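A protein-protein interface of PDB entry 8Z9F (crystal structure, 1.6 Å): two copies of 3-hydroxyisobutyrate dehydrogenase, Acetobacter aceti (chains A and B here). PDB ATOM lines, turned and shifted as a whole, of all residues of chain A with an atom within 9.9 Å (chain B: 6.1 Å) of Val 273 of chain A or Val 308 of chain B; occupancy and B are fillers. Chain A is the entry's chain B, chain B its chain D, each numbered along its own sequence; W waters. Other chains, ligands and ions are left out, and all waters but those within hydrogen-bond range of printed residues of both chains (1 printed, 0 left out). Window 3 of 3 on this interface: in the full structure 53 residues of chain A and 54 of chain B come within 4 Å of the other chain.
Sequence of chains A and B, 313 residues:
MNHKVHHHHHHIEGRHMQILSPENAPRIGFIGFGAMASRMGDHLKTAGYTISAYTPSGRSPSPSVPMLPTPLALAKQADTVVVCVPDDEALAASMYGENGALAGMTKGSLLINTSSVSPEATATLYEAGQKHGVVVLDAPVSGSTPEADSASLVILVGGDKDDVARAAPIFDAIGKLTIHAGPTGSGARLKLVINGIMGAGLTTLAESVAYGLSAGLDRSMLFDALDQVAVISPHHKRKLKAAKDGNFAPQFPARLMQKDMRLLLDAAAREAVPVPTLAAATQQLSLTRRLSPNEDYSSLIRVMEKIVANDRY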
ATOM      1  N   LEU A 264       3.635   9.596 -24.777  1.00  0.00           N
ATOM      2  CA  LEU A 264       4.631   8.548 -25.036  1.00  0.00           C
ATOM      3  C   LEU A 264       4.302   7.265 -24.282  1.00  0.00           C
ATOM      4  O   LEU A 264       4.387   6.165 -24.845  1.00  0.00           O
ATOM      5  CB  LEU A 264       6.023   9.057 -24.652  1.00  0.00           C
ATOM      6  CG  LEU A 264       7.134   8.004 -24.604  1.00  0.00           C
ATOM      7  CD1 LEU A 264       7.363   7.366 -25.956  1.00  0.00           C
ATOM      8  CD2 LEU A 264       8.430   8.669 -24.105  1.00  0.00           C
ATOM      9  N   LEU A 265       3.899   7.376 -23.022  1.00  0.00           N
ATOM     10  CA  LEU A 265       3.623   6.161 -22.272  1.00  0.00           C
ATOM     11  C   LEU A 265       2.346   5.480 -22.768  1.00  0.00           C
ATOM     12  O   LEU A 265       2.258   4.248 -22.764  1.00  0.00           O
ATOM     13  CB  LEU A 265       3.577   6.487 -20.780  1.00  0.00           C
ATOM     14  CG  LEU A 265       4.962   6.422 -20.103  1.00  0.00           C
ATOM     15  CD1 LEU A 265       5.417   4.963 -19.933  1.00  0.00           C
ATOM     16  CD2 LEU A 265       6.088   7.218 -20.813  1.00  0.00           C
ATOM     17  N   ASP A 266       1.366   6.253 -23.233  1.00  0.00           N
ATOM     18  CA  ASP A 266       0.211   5.628 -23.863  1.00  0.00           C
ATOM     19  C   ASP A 266       0.606   4.880 -25.123  1.00  0.00           C
ATOM     20  O   ASP A 266       0.147   3.749 -25.353  1.00  0.00           O
ATOM     21  CB  ASP A 266      -0.862   6.651 -24.204  1.00  0.00           C
ATOM     22  CG  ASP A 266      -2.135   5.984 -24.655  1.00  0.00           C
ATOM     23  OD1 ASP A 266      -2.960   5.620 -23.796  1.00  0.00           O
ATOM     24  OD2 ASP A 266      -2.286   5.796 -25.887  1.00  0.00           O
ATOM     25  N   ALA A 267       1.436   5.496 -25.962  1.00  0.00           N
ATOM     26  CA  ALA A 267       1.831   4.830 -27.200  1.00  0.00           C
ATOM     27  C   ALA A 267       2.681   3.596 -26.910  1.00  0.00           C
ATOM     28  O   ALA A 267       2.538   2.563 -27.580  1.00  0.00           O
ATOM     29  CB  ALA A 267       2.591   5.806 -28.103  1.00  0.00           C
ATOM     30  N   ALA A 268       3.567   3.677 -25.919  1.00  0.00           N
ATOM     31  CA  ALA A 268       4.386   2.518 -25.594  1.00  0.00           C
ATOM     32  C   ALA A 268       3.524   1.374 -25.065  1.00  0.00           C
ATOM     33  O   ALA A 268       3.807   0.208 -25.355  1.00  0.00           O
ATOM     34  CB  ALA A 268       5.470   2.904 -24.583  1.00  0.00           C
ATOM     35  N   ALA A 269       2.445   1.695 -24.349  1.00  0.00           N
ATOM     36  CA  ALA A 269       1.531   0.656 -23.888  1.00  0.00           C
ATOM     37  C   ALA A 269       0.756   0.064 -25.057  1.00  0.00           C
ATOM     38  O   ALA A 269       0.563  -1.154 -25.130  1.00  0.00           O
ATOM     39  CB  ALA A 269       0.591   1.217 -22.816  1.00  0.00           C
ATOM     40  N   ARG A 270       0.324   0.898 -26.008  1.00  0.00           N
ATOM     41  CA  ARG A 270      -0.364   0.341 -27.163  1.00  0.00           C
ATOM     42  C   ARG A 270       0.548  -0.558 -27.987  1.00  0.00           C
ATOM     43  O   ARG A 270       0.064  -1.511 -28.613  1.00  0.00           O
ATOM     44  CB  ARG A 270      -0.922   1.460 -28.035  1.00  0.00           C
ATOM     45  CG  ARG A 270      -2.093   2.156 -27.373  1.00  0.00           C
ATOM     46  CD  ARG A 270      -2.622   3.266 -28.276  1.00  0.00           C
ATOM     47  NE  ARG A 270      -3.747   3.972 -27.669  1.00  0.00           N
ATOM     48  CZ  ARG A 270      -5.021   3.692 -27.907  1.00  0.00           C
ATOM     49  NH1 ARG A 270      -5.374   2.696 -28.706  1.00  0.00           N
ATOM     50  NH2 ARG A 270      -5.969   4.437 -27.341  1.00  0.00           N
ATOM     51  N   GLU A 271       1.850  -0.289 -28.003  1.00  0.00           N
ATOM     52  CA  GLU A 271       2.784  -1.141 -28.728  1.00  0.00           C
ATOM     53  C   GLU A 271       3.300  -2.288 -27.862  1.00  0.00           C
ATOM     54  O   GLU A 271       4.082  -3.113 -28.351  1.00  0.00           O
ATOM     55  CB  GLU A 271       3.982  -0.332 -29.248  1.00  0.00           C
ATOM     56  CG  GLU A 271       3.647   0.888 -30.117  1.00  0.00           C
ATOM     57  CD  GLU A 271       3.089   0.537 -31.476  1.00  0.00           C
ATOM     58  OE1 GLU A 271       2.517   1.444 -32.124  1.00  0.00           O
ATOM     59  OE2 GLU A 271       3.135  -0.658 -31.858  1.00  0.00           O
ATOM     60  N   ALA A 272       2.872  -2.349 -26.596  1.00  0.00           N
ATOM     61  CA  ALA A 272       3.317  -3.348 -25.626  1.00  0.00           C
ATOM     62  C   ALA A 272       4.840  -3.413 -25.529  1.00  0.00           C
ATOM     63  O   ALA A 272       5.433  -4.489 -25.553  1.00  0.00           O
ATOM     64  CB  ALA A 272       2.744  -4.730 -25.957  1.00  0.00           C
ATOM     65  N   VAL A 273       5.475  -2.253 -25.379  1.00  0.00           N
ATOM     66  CA  VAL A 273       6.918  -2.159 -25.174  1.00  0.00           C
ATOM     67  C   VAL A 273       7.163  -1.761 -23.726  1.00  0.00           C
ATOM     68  O   VAL A 273       6.706  -0.692 -23.305  1.00  0.00           O
ATOM     69  CB  VAL A 273       7.582  -1.157 -26.131  1.00  0.00           C
ATOM     70  CG1 VAL A 273       9.102  -1.222 -26.004  1.00  0.00           C
ATOM     71  CG2 VAL A 273       7.181  -1.483 -27.520  1.00  0.00           C
ATOM     72  N   PRO A 274       7.877  -2.570 -22.943  1.00  0.00           N
ATOM     73  CA  PRO A 274       8.159  -2.201 -21.540  1.00  0.00           C
ATOM     74  C   PRO A 274       9.212  -1.103 -21.475  1.00  0.00           C
ATOM     75  O   PRO A 274      10.340  -1.291 -21.935  1.00  0.00           O
ATOM     76  CB  PRO A 274       8.670  -3.506 -20.920  1.00  0.00           C
ATOM     77  CG  PRO A 274       9.101  -4.399 -22.089  1.00  0.00           C
ATOM     78  CD  PRO A 274       8.400  -3.896 -23.325  1.00  0.00           C
ATOM     79  N   VAL A 275       8.853   0.034 -20.874  1.00  0.00           N
ATOM     80  CA  VAL A 275       9.786   1.155 -20.759  1.00  0.00           C
ATOM     81  C   VAL A 275       9.819   1.661 -19.313  1.00  0.00           C
ATOM     82  O   VAL A 275       9.346   2.781 -19.030  1.00  0.00           O
ATOM     83  CB  VAL A 275       9.434   2.268 -21.762  1.00  0.00           C
ATOM     84  CG1 VAL A 275       9.694   1.763 -23.184  1.00  0.00           C
ATOM     85  CG2 VAL A 275       7.968   2.748 -21.649  1.00  0.00           C
ATOM     86  N   PRO A 276      10.420   0.916 -18.382  1.00  0.00           N
ATOM     87  CA  PRO A 276      10.315   1.297 -16.957  1.00  0.00           C
ATOM     88  C   PRO A 276      11.012   2.598 -16.607  1.00  0.00           C
ATOM     89  O   PRO A 276      10.534   3.320 -15.718  1.00  0.00           O
ATOM     90  CB  PRO A 276      10.954   0.115 -16.213  1.00  0.00           C
ATOM     91  CG  PRO A 276      11.799  -0.562 -17.247  1.00  0.00           C
ATOM     92  CD  PRO A 276      11.126  -0.371 -18.565  1.00  0.00           C
ATOM     93  N   THR A 277      12.136   2.916 -17.255  1.00  0.00           N
ATOM     94  CA  THR A 277      12.795   4.185 -16.956  1.00  0.00           C
ATOM     95  C   THR A 277      11.909   5.361 -17.368  1.00  0.00           C
ATOM     96  O   THR A 277      11.766   6.343 -16.624  1.00  0.00           O
ATOM     97  CB  THR A 277      14.167   4.276 -17.636  1.00  0.00           C
ATOM     98  OG1 THR A 277      14.936   3.076 -17.410  1.00  0.00           O
ATOM     99  CG2 THR A 277      14.930   5.440 -17.051  1.00  0.00           C
ATOM    100  N   LEU A 278      11.316   5.289 -18.562  1.00  0.00           N
ATOM    101  CA  LEU A 278      10.443   6.356 -19.026  1.00  0.00           C
ATOM    102  C   LEU A 278       9.201   6.448 -18.155  1.00  0.00           C
ATOM    103  O   LEU A 278       8.690   7.548 -17.921  1.00  0.00           O
ATOM    104  CB  LEU A 278      10.049   6.093 -20.481  1.00  0.00           C
ATOM    105  CG  LEU A 278      11.221   5.973 -21.454  1.00  0.00           C
ATOM    106  CD1 LEU A 278      10.683   5.676 -22.839  1.00  0.00           C
ATOM    107  CD2 LEU A 278      12.053   7.236 -21.473  1.00  0.00           C
ATOM    108  N   ALA A 279       8.690   5.299 -17.700  1.00  0.00           N
ATOM    109  CA  ALA A 279       7.506   5.298 -16.842  1.00  0.00           C
ATOM    110  C   ALA A 279       7.802   5.976 -15.509  1.00  0.00           C
ATOM    111  O   ALA A 279       7.000   6.792 -15.025  1.00  0.00           O
ATOM    112  CB  ALA A 279       7.016   3.856 -16.632  1.00  0.00           C
ATOM    113  N   GLU B 207      15.275   2.469 -24.141  1.00  0.00           N
ATOM    114  CA  GLU B 207      13.820   2.339 -24.106  1.00  0.00           C
ATOM    115  C   GLU B 207      13.163   3.214 -25.157  1.00  0.00           C
ATOM    116  O   GLU B 207      12.149   2.825 -25.761  1.00  0.00           O
ATOM    117  CB  GLU B 207      13.295   2.700 -22.720  1.00  0.00           C
ATOM    118  CG  GLU B 207      13.512   1.582 -21.746  1.00  0.00           C
ATOM    119  CD  GLU B 207      13.357   2.039 -20.334  1.00  0.00           C
ATOM    120  OE1 GLU B 207      12.533   2.950 -20.139  1.00  0.00           O
ATOM    121  OE2 GLU B 207      14.021   1.472 -19.427  1.00  0.00           O
ATOM    122  N   VAL B 209      14.535   4.302 -28.043  1.00  0.00           N
ATOM    123  CA  VAL B 209      14.782   3.641 -29.323  1.00  0.00           C
ATOM    124  C   VAL B 209      13.834   2.467 -29.514  1.00  0.00           C
ATOM    125  O   VAL B 209      13.273   2.271 -30.605  1.00  0.00           O
ATOM    126  CB  VAL B 209      16.257   3.206 -29.408  1.00  0.00           C
ATOM    127  CG1 VAL B 209      16.454   2.266 -30.593  1.00  0.00           C
ATOM    128  CG2 VAL B 209      17.146   4.437 -29.568  1.00  0.00           C
ATOM    129  N   ALA B 210      13.640   1.662 -28.460  1.00  0.00           N
ATOM    130  CA  ALA B 210      12.747   0.507 -28.555  1.00  0.00           C
ATOM    131  C   ALA B 210      11.328   0.930 -28.895  1.00  0.00           C
ATOM    132  O   ALA B 210      10.667   0.288 -29.719  1.00  0.00           O
ATOM    133  CB  ALA B 210      12.752  -0.278 -27.245  1.00  0.00           C
ATOM    134  N   TYR B 211      10.835   2.011 -28.280  1.00  0.00           N
ATOM    135  CA  TYR B 211       9.510   2.484 -28.668  1.00  0.00           C
ATOM    136  C   TYR B 211       9.503   2.864 -30.150  1.00  0.00           C
ATOM    137  O   TYR B 211       8.588   2.489 -30.892  1.00  0.00           O
ATOM    138  CB  TYR B 211       9.042   3.685 -27.813  1.00  0.00           C
ATOM    139  CG  TYR B 211       7.886   4.331 -28.539  1.00  0.00           C
ATOM    140  CD1 TYR B 211       6.642   3.684 -28.589  1.00  0.00           C
ATOM    141  CD2 TYR B 211       8.060   5.494 -29.299  1.00  0.00           C
ATOM    142  CE1 TYR B 211       5.592   4.205 -29.338  1.00  0.00           C
ATOM    143  CE2 TYR B 211       7.018   6.012 -30.058  1.00  0.00           C
ATOM    144  CZ  TYR B 211       5.787   5.365 -30.058  1.00  0.00           C
ATOM    145  OH  TYR B 211       4.762   5.886 -30.819  1.00  0.00           O
ATOM    146  N   LEU B 213      11.289   1.873 -32.705  1.00  0.00           N
ATOM    147  CA  LEU B 213      11.295   0.694 -33.576  1.00  0.00           C
ATOM    148  C   LEU B 213       9.974  -0.050 -33.526  1.00  0.00           C
ATOM    149  O   LEU B 213       9.493  -0.545 -34.561  1.00  0.00           O
ATOM    150  CB  LEU B 213      12.435  -0.250 -33.175  1.00  0.00           C
ATOM    151  CG  LEU B 213      13.833   0.372 -33.250  1.00  0.00           C
ATOM    152  CD1 LEU B 213      14.855  -0.525 -32.534  1.00  0.00           C
ATOM    153  CD2 LEU B 213      14.242   0.634 -34.687  1.00  0.00           C
ATOM    154  N   SER B 214       9.385  -0.176 -32.328  1.00  0.00           N
ATOM    155  CA  SER B 214       8.114  -0.879 -32.192  1.00  0.00           C
ATOM    156  C   SER B 214       7.006  -0.186 -32.958  1.00  0.00           C
ATOM    157  O   SER B 214       6.047  -0.841 -33.398  1.00  0.00           O
ATOM    158  CB  SER B 214       7.729  -0.971 -30.726  1.00  0.00           C
ATOM    159  OG  SER B 214       7.186   0.270 -30.241  1.00  0.00           O
ATOM    160  N   VAL B 303      19.431  -5.650 -26.413  1.00  0.00           N
ATOM    161  CA  VAL B 303      18.406  -6.376 -25.656  1.00  0.00           C
ATOM    162  C   VAL B 303      17.019  -5.847 -25.995  1.00  0.00           C
ATOM    163  O   VAL B 303      16.085  -6.612 -26.257  1.00  0.00           O
ATOM    164  CB  VAL B 303      18.677  -6.266 -24.146  1.00  0.00           C
ATOM    165  CG1 VAL B 303      17.501  -6.870 -23.354  1.00  0.00           C
ATOM    166  CG2 VAL B 303      19.987  -6.948 -23.776  1.00  0.00           C
ATOM    167  N   MET B 304      16.865  -4.529 -25.950  1.00  0.00           N
ATOM    168  CA  MET B 304      15.570  -3.909 -26.189  1.00  0.00           C
ATOM    169  C   MET B 304      15.140  -4.109 -27.639  1.00  0.00           C
ATOM    170  O   MET B 304      13.957  -4.322 -27.924  1.00  0.00           O
ATOM    171  CB  MET B 304      15.692  -2.428 -25.861  1.00  0.00           C
ATOM    172  CG  MET B 304      15.502  -2.007 -24.402  1.00  0.00           C
ATOM    173  SD  MET B 304      14.400  -2.866 -23.295  1.00  0.00           S
ATOM    174  CE  MET B 304      12.868  -2.034 -23.713  1.00  0.00           C
ATOM    175  N   GLU B 305      16.090  -4.028 -28.576  1.00  0.00           N
ATOM    176  CA  GLU B 305      15.755  -4.308 -29.975  1.00  0.00           C
ATOM    177  C   GLU B 305      15.215  -5.720 -30.136  1.00  0.00           C
ATOM    178  O   GLU B 305      14.303  -5.953 -30.937  1.00  0.00           O
ATOM    179  CB  GLU B 305      16.973  -4.118 -30.883  1.00  0.00           C
ATOM    180  CG  GLU B 305      17.461  -2.693 -31.007  1.00  0.00           C
ATOM    181  CD  GLU B 305      18.395  -2.545 -32.200  1.00  0.00           C
ATOM    182  OE1 GLU B 305      17.916  -2.619 -33.351  1.00  0.00           O
ATOM    183  OE2 GLU B 305      19.609  -2.400 -31.972  1.00  0.00           O
ATOM    184  N   LYS B 306      15.785  -6.673 -29.399  1.00  0.00           N
ATOM    185  CA  LYS B 306      15.335  -8.059 -29.497  1.00  0.00           C
ATOM    186  C   LYS B 306      13.940  -8.231 -28.907  1.00  0.00           C
ATOM    187  O   LYS B 306      13.124  -8.998 -29.436  1.00  0.00           O
ATOM    188  CB  LYS B 306      16.338  -8.980 -28.800  1.00  0.00           C
ATOM    189  CG  LYS B 306      15.977 -10.463 -28.876  1.00  0.00           C
ATOM    190  CD  LYS B 306      17.133 -11.356 -28.461  1.00  0.00           C
ATOM    191  CE  LYS B 306      16.749 -12.832 -28.603  1.00  0.00           C
ATOM    192  NZ  LYS B 306      17.671 -13.765 -27.883  1.00  0.00           N
ATOM    193  N   ILE B 307      13.645  -7.527 -27.808  1.00  0.00           N
ATOM    194  CA  ILE B 307      12.301  -7.585 -27.240  1.00  0.00           C
ATOM    195  C   ILE B 307      11.273  -7.136 -28.269  1.00  0.00           C
ATOM    196  O   ILE B 307      10.224  -7.763 -28.433  1.00  0.00           O
ATOM    197  CB  ILE B 307      12.223  -6.733 -25.953  1.00  0.00           C
ATOM    198  CG1 ILE B 307      13.012  -7.408 -24.824  1.00  0.00           C
ATOM    199  CG2 ILE B 307      10.770  -6.494 -25.564  1.00  0.00           C
ATOM    200  CD1 ILE B 307      13.186  -6.536 -23.555  1.00  0.00           C
ATOM    201  N   VAL B 308      11.552  -6.049 -28.986  1.00  0.00           N
ATOM    202  CA  VAL B 308      10.524  -5.543 -29.890  1.00  0.00           C
ATOM    203  C   VAL B 308      10.488  -6.333 -31.192  1.00  0.00           C
ATOM    204  O   VAL B 308       9.437  -6.370 -31.853  1.00  0.00           O
ATOM    205  CB  VAL B 308      10.693  -4.023 -30.117  1.00  0.00           C
ATOM    206  CG1 VAL B 308      10.370  -3.251 -28.823  1.00  0.00           C
ATOM    207  CG2 VAL B 308      12.066  -3.686 -30.622  1.00  0.00           C
ATOM    208  N   ALA B 309      11.586  -7.007 -31.558  1.00  0.00           N
ATOM    209  CA  ALA B 309      11.547  -7.900 -32.710  1.00  0.00           C
ATOM    210  C   ALA B 309      10.613  -9.071 -32.454  1.00  0.00           C
ATOM    211  O   ALA B 309      10.037  -9.629 -33.392  1.00  0.00           O
ATOM    212  CB  ALA B 309      12.950  -8.416 -33.037  1.00  0.00           C
ATOM    213  N   ASN B 310      10.459  -9.456 -31.197  1.00  0.00           N
ATOM    214  CA  ASN B 310       9.536 -10.502 -30.811  1.00  0.00           C
ATOM    215  C   ASN B 310       8.313  -9.884 -30.117  1.00  0.00           C
ATOM    216  O   ASN B 310       7.573 -10.555 -29.398  1.00  0.00           O
ATOM    217  CB  ASN B 310      10.267 -11.507 -29.926  1.00  0.00           C
ATOM    218  CG  ASN B 310      11.467 -12.126 -30.633  1.00  0.00           C
ATOM    219  OD1 ASN B 310      12.624 -11.838 -30.304  1.00  0.00           O
ATOM    220  ND2 ASN B 310      11.194 -12.971 -31.623  1.00  0.00           N
HETATM  221  O   HOH W   1       2.681   4.177 -31.530  1.00  0.00           O
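Of the 16 printed residues of chain A, 10 touch a printed residue of chain B. Of the 14 printed residues of chain B, 6 touch a printed residue of chain A. Printed residues of chain B that touch a printed residue of chain A: Glu 207, Ala 210, Tyr 211, Ser 214, Met 304 and Val 308. Hydrophobic or aromatic side chains of chain B within 4 Å of the printed part of chain A: Ala 210, Tyr 211, Met 304 and Val 308. Among the printed residues, 13 pairs touch across the chains.
The backbone carbonyl oxygen (O) of Ala 268 of chain A sits at hydrogen-bond distance from the backbone NH (N) of Val 273 of chain A, at 3.0 Å. The side-chain hydroxyl of Ser 214 of chain B lies within hydrogen-bond range of the backbone carbonyl oxygen of Tyr 211 of chain B.
Of chain B, only Ala 210 (3.97 Å), Ser 214 (3.2 Å) and Val 308 (3.7 Å) come within 4 Å of Val 273 of chain A. Printed residues of chain A within 4 Å of Val 308 of chain B: Val 273 (3.7 Å). No residue of chain A comes within 4 Å of Ala 309 of chain B. Of the printed residues of chain B, Leu 278 of chain A touches Glu 207 (3.1 Å). Printed residues of chain B within 4 Å of Ala 268 of chain A: Tyr 211. Printed residues of chain B within 4 Å of Ala 267 of chain A: Tyr 211. Printed residues of chain B within 4 Å of Glu 271 of chain A: Tyr 211 (3.9 Å) and Ser 214 (3.3 Å). Ala 279 of chain A touches none of the printed residues of chain B. The nearest residue of chain B that does not touch Val 273 of chain A is Tyr 211 of chain B (4.3 Å). The nearest residue of chain A that does not touch Val 308 of chain B is Pro 274 of chain A (5.9 Å). The nearest printed residue of chain B that does not touch Pro 274 of chain A is Ile 307 of chain B (4.2 Å).
Water W1 lies within hydrogen-bond range of the side-chain hydroxyl of Tyr 211 of chain B (2.8 Å) and the side-chain carboxylate of Glu 271 of chain A (2.8 Å).
No position is printed for both chains. Of the 13 pairs that touch across the chains among the printed residues, none has its exchanged pair printed and touching as well.
Leu 264 of chain A touches Tyr 211 of chain B (CD1 to CD2, 3.9 Å). Tyr 211 of chain B touches Ala 267 of chain A (OH to CB, 3.5 Å). Ala 268 of chain A touches Tyr 211 of chain B. CE1 of Tyr 211 of chain B touches CG of Glu 271 of chain A, 3.9 Å away. Val 273 of chain A touches Ala 210 of chain B (CG1 to CB, 3.97 Å). Val 273 of chain A touches Ser 214 of chain B. CG1 of Val 273 of chain A touches CG1 of Val 308 of chain B, at 3.7 Å. O of Pro 274 of chain A touches CE of Met 304 of chain B, 3.2 Å away.
The backbone nitrogen (N) of Pro 276 of chain A sits close to the side-chain carboxylate (OE1) of Glu 207 of chain B (3.4 Å). OE2 of Glu 207 of chain B is in hydrogen-bond range of OG1 of Thr 277 of chain A (2.7 Å). N of Leu 278 of chain A lies within hydrogen-bond range of OE1 of Glu 207 of chain B, 3.1 Å away. O of Ser 214 of chain B sits close to OE2 of Glu 271 of chain A (3.3 Å). The side-chain carboxylate of Glu 207 of chain B lies close to the backbone carbonyl oxygen of Val 275 of chain A, at 3.4 Å.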
